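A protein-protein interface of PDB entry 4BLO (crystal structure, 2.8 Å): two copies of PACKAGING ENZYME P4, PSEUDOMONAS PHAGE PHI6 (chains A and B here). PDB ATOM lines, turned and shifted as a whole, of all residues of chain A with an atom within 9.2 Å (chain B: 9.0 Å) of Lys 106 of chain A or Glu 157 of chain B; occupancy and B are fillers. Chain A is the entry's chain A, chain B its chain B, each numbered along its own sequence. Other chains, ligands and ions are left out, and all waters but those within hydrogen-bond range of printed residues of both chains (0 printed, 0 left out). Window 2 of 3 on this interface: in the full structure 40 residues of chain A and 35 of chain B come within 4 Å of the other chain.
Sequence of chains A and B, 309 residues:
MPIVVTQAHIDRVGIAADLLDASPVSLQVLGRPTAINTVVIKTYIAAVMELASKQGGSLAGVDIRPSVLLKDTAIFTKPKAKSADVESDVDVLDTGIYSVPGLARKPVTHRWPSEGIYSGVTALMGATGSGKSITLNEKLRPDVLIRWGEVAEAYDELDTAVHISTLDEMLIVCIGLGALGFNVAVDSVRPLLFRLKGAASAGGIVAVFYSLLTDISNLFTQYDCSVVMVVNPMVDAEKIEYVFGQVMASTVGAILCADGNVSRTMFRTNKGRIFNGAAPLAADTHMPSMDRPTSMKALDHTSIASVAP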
ATOM      1  N   LEU A  19       6.971  17.021  16.574  1.00  0.00           N
ATOM      2  CA  LEU A  19       8.323  17.117  17.110  1.00  0.00           C
ATOM      3  C   LEU A  19       9.314  16.342  16.259  1.00  0.00           C
ATOM      4  O   LEU A  19      10.407  16.847  15.987  1.00  0.00           O
ATOM      5  CB  LEU A  19       8.380  16.604  18.560  1.00  0.00           C
ATOM      6  CG  LEU A  19       7.753  17.483  19.639  1.00  0.00           C
ATOM      7  CD1 LEU A  19       7.427  16.660  20.857  1.00  0.00           C
ATOM      8  CD2 LEU A  19       8.646  18.676  20.005  1.00  0.00           C
ATOM      9  N   GLY A 102      20.846  21.639  20.195  1.00  0.00           N
ATOM     10  CA  GLY A 102      20.107  22.012  21.390  1.00  0.00           C
ATOM     11  C   GLY A 102      18.763  22.638  21.064  1.00  0.00           C
ATOM     12  O   GLY A 102      18.473  22.926  19.898  1.00  0.00           O
ATOM     13  N   LEU A 103      17.933  22.836  22.107  1.00  0.00           N
ATOM     14  CA  LEU A 103      16.608  23.435  22.002  1.00  0.00           C
ATOM     15  C   LEU A 103      16.658  24.949  22.257  1.00  0.00           C
ATOM     16  O   LEU A 103      17.095  25.390  23.325  1.00  0.00           O
ATOM     17  CB  LEU A 103      15.638  22.778  22.992  1.00  0.00           C
ATOM     18  CG  LEU A 103      14.522  21.887  22.456  1.00  0.00           C
ATOM     19  CD1 LEU A 103      13.528  21.610  23.539  1.00  0.00           C
ATOM     20  CD2 LEU A 103      13.790  22.500  21.272  1.00  0.00           C
ATOM     21  N   ALA A 104      16.199  25.735  21.284  1.00  0.00           N
ATOM     22  CA  ALA A 104      16.158  27.186  21.400  1.00  0.00           C
ATOM     23  C   ALA A 104      15.087  27.626  22.424  1.00  0.00           C
ATOM     24  O   ALA A 104      15.260  28.638  23.107  1.00  0.00           O
ATOM     25  CB  ALA A 104      15.877  27.799  20.048  1.00  0.00           C
ATOM     26  N   ARG A 105      13.994  26.854  22.531  1.00  0.00           N
ATOM     27  CA  ARG A 105      12.911  27.106  23.470  1.00  0.00           C
ATOM     28  C   ARG A 105      13.231  26.475  24.840  1.00  0.00           C
ATOM     29  O   ARG A 105      14.232  25.754  24.973  1.00  0.00           O
ATOM     30  CB  ARG A 105      11.576  26.566  22.907  1.00  0.00           C
ATOM     31  CG  ARG A 105      11.581  25.097  22.547  1.00  0.00           C
ATOM     32  CD  ARG A 105      10.206  24.544  22.246  1.00  0.00           C
ATOM     33  NE  ARG A 105      10.247  23.094  22.017  1.00  0.00           N
ATOM     34  CZ  ARG A 105      10.106  22.183  22.976  1.00  0.00           C
ATOM     35  NH1 ARG A 105       9.929  22.560  24.237  1.00  0.00           N
ATOM     36  NH2 ARG A 105      10.162  20.887  22.684  1.00  0.00           N
ATOM     37  N   LYS A 106      12.382  26.756  25.853  1.00  0.00           N
ATOM     38  CA  LYS A 106      12.493  26.171  27.190  1.00  0.00           C
ATOM     39  C   LYS A 106      12.091  24.692  27.099  1.00  0.00           C
ATOM     40  O   LYS A 106      11.079  24.400  26.453  1.00  0.00           O
ATOM     41  CB  LYS A 106      11.594  26.932  28.190  1.00  0.00           C
ATOM     42  CG  LYS A 106      11.793  26.529  29.650  1.00  0.00           C
ATOM     43  CD  LYS A 106      11.600  27.704  30.601  1.00  0.00           C
ATOM     44  CE  LYS A 106      12.179  27.413  31.967  1.00  0.00           C
ATOM     45  NZ  LYS A 106      12.326  28.646  32.789  1.00  0.00           N
ATOM     46  N   PRO A 107      12.858  23.730  27.671  1.00  0.00           N
ATOM     47  CA  PRO A 107      12.438  22.322  27.569  1.00  0.00           C
ATOM     48  C   PRO A 107      11.222  22.032  28.441  1.00  0.00           C
ATOM     49  O   PRO A 107      11.018  22.699  29.468  1.00  0.00           O
ATOM     50  CB  PRO A 107      13.664  21.527  28.042  1.00  0.00           C
ATOM     51  CG  PRO A 107      14.709  22.522  28.367  1.00  0.00           C
ATOM     52  CD  PRO A 107      14.084  23.863  28.477  1.00  0.00           C
ATOM     53  N   VAL A 108      10.378  21.086  27.990  1.00  0.00           N
ATOM     54  CA  VAL A 108       9.217  20.590  28.731  1.00  0.00           C
ATOM     55  C   VAL A 108       9.750  20.008  30.052  1.00  0.00           C
ATOM     56  O   VAL A 108      10.743  19.268  30.035  1.00  0.00           O
ATOM     57  CB  VAL A 108       8.429  19.525  27.890  1.00  0.00           C
ATOM     58  CG1 VAL A 108       7.617  18.550  28.763  1.00  0.00           C
ATOM     59  CG2 VAL A 108       7.558  20.189  26.832  1.00  0.00           C
ATOM     60  N   THR A 109       9.114  20.373  31.180  1.00  0.00           N
ATOM     61  CA  THR A 109       9.472  19.879  32.506  1.00  0.00           C
ATOM     62  C   THR A 109       8.701  18.595  32.798  1.00  0.00           C
ATOM     63  O   THR A 109       7.705  18.315  32.133  1.00  0.00           O
ATOM     64  CB  THR A 109       9.266  20.953  33.575  1.00  0.00           C
ATOM     65  OG1 THR A 109       7.964  21.531  33.445  1.00  0.00           O
ATOM     66  CG2 THR A 109      10.339  22.034  33.514  1.00  0.00           C
ATOM     67  N   GLY A 116      10.177  18.961  38.527  1.00  0.00           N
ATOM     68  CA  GLY A 116      10.490  20.051  37.613  1.00  0.00           C
ATOM     69  C   GLY A 116      11.697  19.839  36.717  1.00  0.00           C
ATOM     70  O   GLY A 116      12.161  20.796  36.087  1.00  0.00           O
ATOM     71  N   TYR A 118      14.056  19.027  33.560  1.00  0.00           N
ATOM     72  CA  TYR A 118      13.921  19.264  32.127  1.00  0.00           C
ATOM     73  C   TYR A 118      13.982  17.937  31.373  1.00  0.00           C
ATOM     74  O   TYR A 118      14.505  16.943  31.899  1.00  0.00           O
ATOM     75  CB  TYR A 118      15.015  20.219  31.615  1.00  0.00           C
ATOM     76  CG  TYR A 118      14.914  21.649  32.117  1.00  0.00           C
ATOM     77  CD1 TYR A 118      13.706  22.338  32.084  1.00  0.00           C
ATOM     78  CD2 TYR A 118      16.048  22.350  32.513  1.00  0.00           C
ATOM     79  CE1 TYR A 118      13.610  23.658  32.524  1.00  0.00           C
ATOM     80  CE2 TYR A 118      15.971  23.678  32.931  1.00  0.00           C
ATOM     81  CZ  TYR A 118      14.747  24.325  32.949  1.00  0.00           C
ATOM     82  OH  TYR A 118      14.665  25.626  33.388  1.00  0.00           O
ATOM     83  N   SER A 119      13.441  17.914  30.148  1.00  0.00           N
ATOM     84  CA  SER A 119      13.484  16.734  29.292  1.00  0.00           C
ATOM     85  C   SER A 119      14.927  16.458  28.898  1.00  0.00           C
ATOM     86  O   SER A 119      15.692  17.402  28.672  1.00  0.00           O
ATOM     87  CB  SER A 119      12.620  16.931  28.058  1.00  0.00           C
ATOM     88  OG  SER A 119      11.268  17.181  28.426  1.00  0.00           O
ATOM     89  N   THR A 221      15.671  15.753  24.962  1.00  0.00           N
ATOM     90  CA  THR A 221      15.256  17.141  25.259  1.00  0.00           C
ATOM     91  C   THR A 221      14.401  17.693  24.110  1.00  0.00           C
ATOM     92  O   THR A 221      13.378  18.336  24.349  1.00  0.00           O
ATOM     93  CB  THR A 221      16.470  18.033  25.530  1.00  0.00           C
ATOM     94  OG1 THR A 221      17.316  17.405  26.504  1.00  0.00           O
ATOM     95  CG2 THR A 221      16.083  19.431  25.994  1.00  0.00           C
ATOM     96  N   GLN A 222      14.801  17.389  22.875  1.00  0.00           N
ATOM     97  CA  GLN A 222      14.120  17.798  21.658  1.00  0.00           C
ATOM     98  C   GLN A 222      12.761  17.117  21.479  1.00  0.00           C
ATOM     99  O   GLN A 222      11.864  17.724  20.894  1.00  0.00           O
ATOM    100  CB  GLN A 222      15.004  17.479  20.456  1.00  0.00           C
ATOM    101  CG  GLN A 222      14.900  18.540  19.380  1.00  0.00           C
ATOM    102  CD  GLN A 222      16.099  18.514  18.482  1.00  0.00           C
ATOM    103  OE1 GLN A 222      16.316  17.563  17.728  1.00  0.00           O
ATOM    104  NE2 GLN A 222      16.899  19.565  18.543  1.00  0.00           N
ATOM    105  N   ASP A 224      10.868  15.881  24.122  1.00  0.00           N
ATOM    106  CA  ASP A 224      10.212  16.030  25.432  1.00  0.00           C
ATOM    107  C   ASP A 224      10.157  14.732  26.254  1.00  0.00           C
ATOM    108  O   ASP A 224       9.171  14.509  26.974  1.00  0.00           O
ATOM    109  CB  ASP A 224       8.791  16.605  25.278  1.00  0.00           C
ATOM    110  CG  ASP A 224       8.660  17.894  24.492  1.00  0.00           C
ATOM    111  OD1 ASP A 224       9.612  18.723  24.533  1.00  0.00           O
ATOM    112  OD2 ASP A 224       7.580  18.122  23.925  1.00  0.00           O
ATOM    113  N   ARG A 268      18.841  18.985  36.629  1.00  0.00           N
ATOM    114  CA  ARG A 268      18.653  20.289  35.996  1.00  0.00           C
ATOM    115  C   ARG A 268      17.148  20.536  35.906  1.00  0.00           C
ATOM    116  O   ARG A 268      16.469  19.936  35.057  1.00  0.00           O
ATOM    117  CB  ARG A 268      19.322  20.334  34.620  1.00  0.00           C
ATOM    118  CG  ARG A 268      20.832  20.269  34.671  1.00  0.00           C
ATOM    119  CD  ARG A 268      21.422  20.238  33.283  1.00  0.00           C
ATOM    120  NE  ARG A 268      22.789  19.714  33.299  1.00  0.00           N
ATOM    121  CZ  ARG A 268      23.881  20.461  33.392  1.00  0.00           C
ATOM    122  NH1 ARG A 268      23.786  21.781  33.474  1.00  0.00           N
ATOM    123  NH2 ARG A 268      25.076  19.894  33.411  1.00  0.00           N
ATOM    124  N   THR A 269      16.614  21.349  36.840  1.00  0.00           N
ATOM    125  CA  THR A 269      15.179  21.629  36.931  1.00  0.00           C
ATOM    126  C   THR A 269      14.824  23.083  36.559  1.00  0.00           C
ATOM    127  O   THR A 269      15.710  23.897  36.320  1.00  0.00           O
ATOM    128  CB  THR A 269      14.667  21.310  38.356  1.00  0.00           C
ATOM    129  OG1 THR A 269      15.079  22.339  39.263  1.00  0.00           O
ATOM    130  CG2 THR A 269      15.103  19.925  38.853  1.00  0.00           C
ATOM    131  N   ASN A 270      13.513  23.399  36.540  1.00  0.00           N
ATOM    132  CA  ASN A 270      12.979  24.741  36.272  1.00  0.00           C
ATOM    133  C   ASN A 270      13.327  25.695  37.427  1.00  0.00           C
ATOM    134  O   ASN A 270      13.336  26.914  37.245  1.00  0.00           O
ATOM    135  CB  ASN A 270      11.460  24.700  36.048  1.00  0.00           C
ATOM    136  CG  ASN A 270      10.662  23.865  37.037  1.00  0.00           C
ATOM    137  OD1 ASN A 270      11.056  23.642  38.190  1.00  0.00           O
ATOM    138  ND2 ASN A 270       9.504  23.393  36.601  1.00  0.00           N
ATOM    139  N   LYS A 271      13.623  25.115  38.612  1.00  0.00           N
ATOM    140  CA  LYS A 271      14.052  25.798  39.834  1.00  0.00           C
ATOM    141  C   LYS A 271      15.602  25.896  39.886  1.00  0.00           C
ATOM    142  O   LYS A 271      16.147  26.447  40.841  1.00  0.00           O
ATOM    143  CB  LYS A 271      13.495  25.079  41.084  1.00  0.00           C
ATOM    144  CG  LYS A 271      11.958  25.060  41.181  1.00  0.00           C
ATOM    145  CD  LYS A 271      11.357  26.329  41.833  1.00  0.00           C
ATOM    146  CE  LYS A 271       9.847  26.356  41.818  1.00  0.00           C
ATOM    147  NZ  LYS A 271       9.281  25.442  42.845  1.00  0.00           N
ATOM    148  N   GLY A 272      16.273  25.392  38.844  1.00  0.00           N
ATOM    149  CA  GLY A 272      17.727  25.416  38.687  1.00  0.00           C
ATOM    150  C   GLY A 272      18.422  24.070  38.826  1.00  0.00           C
ATOM    151  O   GLY A 272      17.759  23.050  39.031  1.00  0.00           O
ATOM    152  N   MET B   1      20.315  39.995  25.146  1.00  0.00           N
ATOM    153  CA  MET B   1      19.811  38.821  24.430  1.00  0.00           C
ATOM    154  C   MET B   1      19.777  39.002  22.873  1.00  0.00           C
ATOM    155  O   MET B   1      20.134  38.023  22.229  1.00  0.00           O
ATOM    156  CB  MET B   1      18.426  38.401  24.937  1.00  0.00           C
ATOM    157  CG  MET B   1      18.444  37.172  25.833  1.00  0.00           C
ATOM    158  SD  MET B   1      16.748  36.668  26.251  1.00  0.00           S
ATOM    159  CE  MET B   1      17.059  35.423  27.507  1.00  0.00           C
ATOM    160  N   PRO B   2      19.408  40.145  22.205  1.00  0.00           N
ATOM    161  CA  PRO B   2      19.382  40.133  20.722  1.00  0.00           C
ATOM    162  C   PRO B   2      20.746  40.332  20.054  1.00  0.00           C
ATOM    163  O   PRO B   2      21.712  40.680  20.718  1.00  0.00           O
ATOM    164  CB  PRO B   2      18.426  41.268  20.372  1.00  0.00           C
ATOM    165  CG  PRO B   2      18.485  42.184  21.518  1.00  0.00           C
ATOM    166  CD  PRO B   2      18.926  41.436  22.738  1.00  0.00           C
ATOM    167  N   ALA B  60      17.522  37.393  15.813  1.00  0.00           N
ATOM    168  CA  ALA B  60      17.455  36.292  16.776  1.00  0.00           C
ATOM    169  C   ALA B  60      18.430  35.177  16.348  1.00  0.00           C
ATOM    170  O   ALA B  60      18.413  34.751  15.186  1.00  0.00           O
ATOM    171  CB  ALA B  60      16.039  35.757  16.875  1.00  0.00           C
ATOM    172  N   GLY B  61      19.277  34.744  17.280  1.00  0.00           N
ATOM    173  CA  GLY B  61      20.279  33.693  17.073  1.00  0.00           C
ATOM    174  C   GLY B  61      19.738  32.453  16.405  1.00  0.00           C
ATOM    175  O   GLY B  61      20.433  31.829  15.602  1.00  0.00           O
ATOM    176  N   VAL B  62      18.474  32.118  16.713  1.00  0.00           N
ATOM    177  CA  VAL B  62      17.729  30.987  16.160  1.00  0.00           C
ATOM    178  C   VAL B  62      17.545  31.155  14.651  1.00  0.00           C
ATOM    179  O   VAL B  62      17.600  30.171  13.925  1.00  0.00           O
ATOM    180  CB  VAL B  62      16.339  30.825  16.843  1.00  0.00           C
ATOM    181  CG1 VAL B  62      15.864  29.380  16.769  1.00  0.00           C
ATOM    182  CG2 VAL B  62      16.364  31.301  18.287  1.00  0.00           C
ATOM    183  N   LEU B 145      26.547  33.572  20.694  1.00  0.00           N
ATOM    184  CA  LEU B 145      26.884  32.392  21.480  1.00  0.00           C
ATOM    185  C   LEU B 145      26.530  31.112  20.708  1.00  0.00           C
ATOM    186  O   LEU B 145      25.356  30.747  20.587  1.00  0.00           O
ATOM    187  CB  LEU B 145      26.202  32.426  22.867  1.00  0.00           C
ATOM    188  CG  LEU B 145      26.272  31.143  23.724  1.00  0.00           C
ATOM    189  CD1 LEU B 145      27.659  30.909  24.275  1.00  0.00           C
ATOM    190  CD2 LEU B 145      25.248  31.176  24.846  1.00  0.00           C
ATOM    191  N   ARG B 147      26.246  27.303  20.429  1.00  0.00           N
ATOM    192  CA  ARG B 147      26.046  26.187  21.348  1.00  0.00           C
ATOM    193  C   ARG B 147      26.156  24.858  20.593  1.00  0.00           C
ATOM    194  O   ARG B 147      25.426  24.620  19.624  1.00  0.00           O
ATOM    195  CB  ARG B 147      24.729  26.326  22.106  1.00  0.00           C
ATOM    196  CG  ARG B 147      24.846  27.312  23.267  1.00  0.00           C
ATOM    197  CD  ARG B 147      24.252  26.706  24.527  1.00  0.00           C
ATOM    198  NE  ARG B 147      25.254  26.392  25.546  1.00  0.00           N
ATOM    199  CZ  ARG B 147      25.087  25.505  26.523  1.00  0.00           C
ATOM    200  NH1 ARG B 147      23.966  24.802  26.607  1.00  0.00           N
ATOM    201  NH2 ARG B 147      26.051  25.292  27.404  1.00  0.00           N
ATOM    202  N   VAL B 151      24.685  19.958  27.011  1.00  0.00           N
ATOM    203  CA  VAL B 151      23.356  19.548  27.447  1.00  0.00           C
ATOM    204  C   VAL B 151      22.451  20.799  27.667  1.00  0.00           C
ATOM    205  O   VAL B 151      22.955  21.929  27.654  1.00  0.00           O
ATOM    206  CB  VAL B 151      23.481  18.620  28.681  1.00  0.00           C
ATOM    207  CG1 VAL B 151      23.492  19.394  30.000  1.00  0.00           C
ATOM    208  CG2 VAL B 151      22.406  17.553  28.673  1.00  0.00           C
ATOM    209  N   ALA B 152      21.121  20.590  27.810  1.00  0.00           N
ATOM    210  CA  ALA B 152      20.141  21.671  27.988  1.00  0.00           C
ATOM    211  C   ALA B 152      20.446  22.522  29.235  1.00  0.00           C
ATOM    212  O   ALA B 152      20.435  22.023  30.369  1.00  0.00           O
ATOM    213  CB  ALA B 152      18.728  21.110  28.060  1.00  0.00           C
ATOM    214  N   GLU B 153      20.781  23.803  28.992  1.00  0.00           N
ATOM    215  CA  GLU B 153      21.099  24.794  30.024  1.00  0.00           C
ATOM    216  C   GLU B 153      20.290  26.086  29.792  1.00  0.00           C
ATOM    217  O   GLU B 153      19.593  26.198  28.773  1.00  0.00           O
ATOM    218  CB  GLU B 153      22.611  25.089  30.028  1.00  0.00           C
ATOM    219  CG  GLU B 153      23.478  23.901  30.410  1.00  0.00           C
ATOM    220  CD  GLU B 153      24.881  24.267  30.841  1.00  0.00           C
ATOM    221  OE1 GLU B 153      25.043  24.676  32.014  1.00  0.00           O
ATOM    222  OE2 GLU B 153      25.814  24.155  30.010  1.00  0.00           O
ATOM    223  N   ALA B 154      20.385  27.060  30.735  1.00  0.00           N
ATOM    224  CA  ALA B 154      19.705  28.366  30.662  1.00  0.00           C
ATOM    225  C   ALA B 154      20.164  29.192  29.449  1.00  0.00           C
ATOM    226  O   ALA B 154      19.402  30.032  28.947  1.00  0.00           O
ATOM    227  CB  ALA B 154      19.957  29.161  31.931  1.00  0.00           C
ATOM    228  N   TYR B 155      21.416  28.956  28.989  1.00  0.00           N
ATOM    229  CA  TYR B 155      22.035  29.679  27.880  1.00  0.00           C
ATOM    230  C   TYR B 155      21.374  29.349  26.536  1.00  0.00           C
ATOM    231  O   TYR B 155      21.505  30.112  25.587  1.00  0.00           O
ATOM    232  CB  TYR B 155      23.544  29.380  27.818  1.00  0.00           C
ATOM    233  CG  TYR B 155      24.210  29.308  29.176  1.00  0.00           C
ATOM    234  CD1 TYR B 155      24.404  30.454  29.944  1.00  0.00           C
ATOM    235  CD2 TYR B 155      24.643  28.093  29.698  1.00  0.00           C
ATOM    236  CE1 TYR B 155      25.008  30.390  31.201  1.00  0.00           C
ATOM    237  CE2 TYR B 155      25.242  28.017  30.956  1.00  0.00           C
ATOM    238  CZ  TYR B 155      25.418  29.168  31.705  1.00  0.00           C
ATOM    239  OH  TYR B 155      26.011  29.086  32.941  1.00  0.00           O
ATOM    240  N   ASP B 156      20.646  28.239  26.463  1.00  0.00           N
ATOM    241  CA  ASP B 156      19.975  27.828  25.235  1.00  0.00           C
ATOM    242  C   ASP B 156      18.723  28.680  24.942  1.00  0.00           C
ATOM    243  O   ASP B 156      18.328  28.783  23.785  1.00  0.00           O
ATOM    244  CB  ASP B 156      19.618  26.330  25.310  1.00  0.00           C
ATOM    245  CG  ASP B 156      20.845  25.441  25.388  1.00  0.00           C
ATOM    246  OD1 ASP B 156      21.463  25.187  24.335  1.00  0.00           O
ATOM    247  OD2 ASP B 156      21.203  25.018  26.510  1.00  0.00           O
ATOM    248  N   GLU B 157      18.123  29.295  25.979  1.00  0.00           N
ATOM    249  CA  GLU B 157      16.919  30.125  25.861  1.00  0.00           C
ATOM    250  C   GLU B 157      17.234  31.587  25.440  1.00  0.00           C
ATOM    251  O   GLU B 157      16.307  32.363  25.154  1.00  0.00           O
ATOM    252  CB  GLU B 157      16.141  30.111  27.178  1.00  0.00           C
ATOM    253  CG  GLU B 157      15.265  28.883  27.336  1.00  0.00           C
ATOM    254  CD  GLU B 157      14.652  28.732  28.714  1.00  0.00           C
ATOM    255  OE1 GLU B 157      13.918  29.652  29.140  1.00  0.00           O
ATOM    256  OE2 GLU B 157      14.887  27.679  29.350  1.00  0.00           O
ATOM    257  N   LEU B 158      18.533  31.938  25.404  1.00  0.00           N
ATOM    258  CA  LEU B 158      19.068  33.247  25.030  1.00  0.00           C
ATOM    259  C   LEU B 158      18.901  33.493  23.536  1.00  0.00           C
ATOM    260  O   LEU B 158      19.068  32.555  22.748  1.00  0.00           O
ATOM    261  CB  LEU B 158      20.568  33.299  25.398  1.00  0.00           C
ATOM    262  CG  LEU B 158      21.001  33.933  26.720  1.00  0.00           C
ATOM    263  CD1 LEU B 158      20.398  33.242  27.910  1.00  0.00           C
ATOM    264  CD2 LEU B 158      22.478  33.844  26.868  1.00  0.00           C
ATOM    265  N   ASP B 159      18.584  34.760  23.143  1.00  0.00           N
ATOM    266  CA  ASP B 159      18.421  35.180  21.743  1.00  0.00           C
ATOM    267  C   ASP B 159      19.778  35.338  21.034  1.00  0.00           C
ATOM    268  O   ASP B 159      19.810  35.619  19.828  1.00  0.00           O
ATOM    269  CB  ASP B 159      17.657  36.510  21.652  1.00  0.00           C
ATOM    270  CG  ASP B 159      16.180  36.494  21.969  1.00  0.00           C
ATOM    271  OD1 ASP B 159      15.618  35.373  22.186  1.00  0.00           O
ATOM    272  OD2 ASP B 159      15.567  37.592  21.972  1.00  0.00           O
ATOM    273  N   THR B 160      20.891  35.245  21.797  1.00  0.00           N
ATOM    274  CA  THR B 160      22.256  35.313  21.269  1.00  0.00           C
ATOM    275  C   THR B 160      22.710  33.901  20.855  1.00  0.00           C
ATOM    276  O   THR B 160      23.646  33.774  20.067  1.00  0.00           O
ATOM    277  CB  THR B 160      23.233  35.925  22.299  1.00  0.00           C
ATOM    278  OG1 THR B 160      23.136  35.218  23.535  1.00  0.00           O
ATOM    279  CG2 THR B 160      23.015  37.398  22.527  1.00  0.00           C
ATOM    280  N   ALA B 161      22.045  32.850  21.399  1.00  0.00           N
ATOM    281  CA  ALA B 161      22.353  31.434  21.173  1.00  0.00           C
ATOM    282  C   ALA B 161      21.995  30.973  19.769  1.00  0.00           C
ATOM    283  O   ALA B 161      20.888  31.208  19.292  1.00  0.00           O
ATOM    284  CB  ALA B 161      21.651  30.553  22.198  1.00  0.00           C
ATOM    285  N   VAL B 162      22.962  30.331  19.112  1.00  0.00           N
ATOM    286  CA  VAL B 162      22.826  29.766  17.767  1.00  0.00           C
ATOM    287  C   VAL B 162      23.283  28.289  17.859  1.00  0.00           C
ATOM    288  O   VAL B 162      24.445  27.994  18.135  1.00  0.00           O
ATOM    289  CB  VAL B 162      23.529  30.598  16.651  1.00  0.00           C
ATOM    290  CG1 VAL B 162      24.914  31.062  17.075  1.00  0.00           C
ATOM    291  CG2 VAL B 162      23.589  29.837  15.333  1.00  0.00           C
ATOM    292  N   HIS B 163      22.317  27.373  17.705  1.00  0.00           N
ATOM    293  CA  HIS B 163      22.511  25.947  17.853  1.00  0.00           C
ATOM    294  C   HIS B 163      22.948  25.302  16.563  1.00  0.00           C
ATOM    295  O   HIS B 163      22.211  25.273  15.570  1.00  0.00           O
ATOM    296  CB  HIS B 163      21.252  25.275  18.402  1.00  0.00           C
ATOM    297  CG  HIS B 163      20.902  25.751  19.768  1.00  0.00           C
ATOM    298  ND1 HIS B 163      19.948  26.736  19.961  1.00  0.00           N
ATOM    299  CD2 HIS B 163      21.431  25.406  20.966  1.00  0.00           C
ATOM    300  CE1 HIS B 163      19.909  26.939  21.267  1.00  0.00           C
ATOM    301  NE2 HIS B 163      20.784  26.157  21.912  1.00  0.00           N
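The backbone carbonyl oxygen (O) of Ala 104 of chain A lies close to the backbone carbonyl oxygen (O) of Asp 156 of chain B. NH1 of Arg 268 of chain A lies within salt-bridge range of OE1 of Glu 153 of chain B.
No position is printed for both chains.
Hydrophobic or aromatic side chains of chain B that line the printed part of chain A: Val 62, Val 151, Ala 152 and His 163.
The side-chain hydroxyl (OG1) of Thr 221 of chain A is in hydrogen-bond range of the backbone carbonyl oxygen (O) of Ser 119 of chain A (2.7 Å). The backbone NH (N) of Tyr 118 of chain A is in hydrogen-bond range of the backbone carbonyl oxygen (O) of Arg 268 of chain A (3.0 Å). OE2 of Glu 153 of chain B lies within salt-bridge range of NH2 of Arg 147 of chain B (2.9 Å). O of Val 151 of chain B lies within hydrogen-bond range of NH1 of Arg 147 of chain B, 3.2 Å away. The backbone NH (N) of Glu 153 of chain B is in hydrogen-bond range of the side-chain carboxylate (OD2) of Asp 156 of chain B (2.8 Å). NH1 of Arg 147 of chain B lies within salt-bridge range of OD2 of Asp 156 of chain B (2.8 Å).
Of chain B, only Glu 157 comes within 4 Å of Lys 106 of chain A. Printed residues of chain A within 4 Å of Glu 157 of chain B: Ala 104, Lys 106 and Pro 107. Printed residues of chain B within 4 Å of Pro 107 of chain A: Glu 157. Printed residues of chain A within 4 Å of Val 151 of chain B: Arg 268. Of the printed residues of chain A, Asp 156 of chain B touches Leu 103 (3.3 Å) and Ala 104 (3.1 Å). Ala 60 of chain B touches none of the printed residues of chain A. The nearest printed residue of chain A that does not touch Glu 157 of chain B is Arg 105 of chain A (4.02 Å).
Among the printed residues, merely in contact across the chains: Lys 106 of chain A with Glu 157 of chain B (3.3 Å), Leu 103 of chain A with Asp 156 of chain B (3.3 Å), Arg 268 of chain A with Val 151 of chain B (3.4 Å), Ala 104 of chain A with Glu 157 of chain B (3.5 Å), Arg 268 of chain A with Ala 152 of chain B (3.6 Å), Ala 104 of chain A with Val 62 of chain B (3.6 Å), Gly 102 of chain A with His 163 of chain B (3.7 Å), Thr 221 of chain A with Ala 152 of chain B (3.8 Å), Ala 104 of chain A with His 163 of chain B (3.8 Å), Leu 103 of chain A with His 163 of chain B (3.8 Å) and Pro 107 of chain A with Glu 157 of chain B (3.996 Å).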
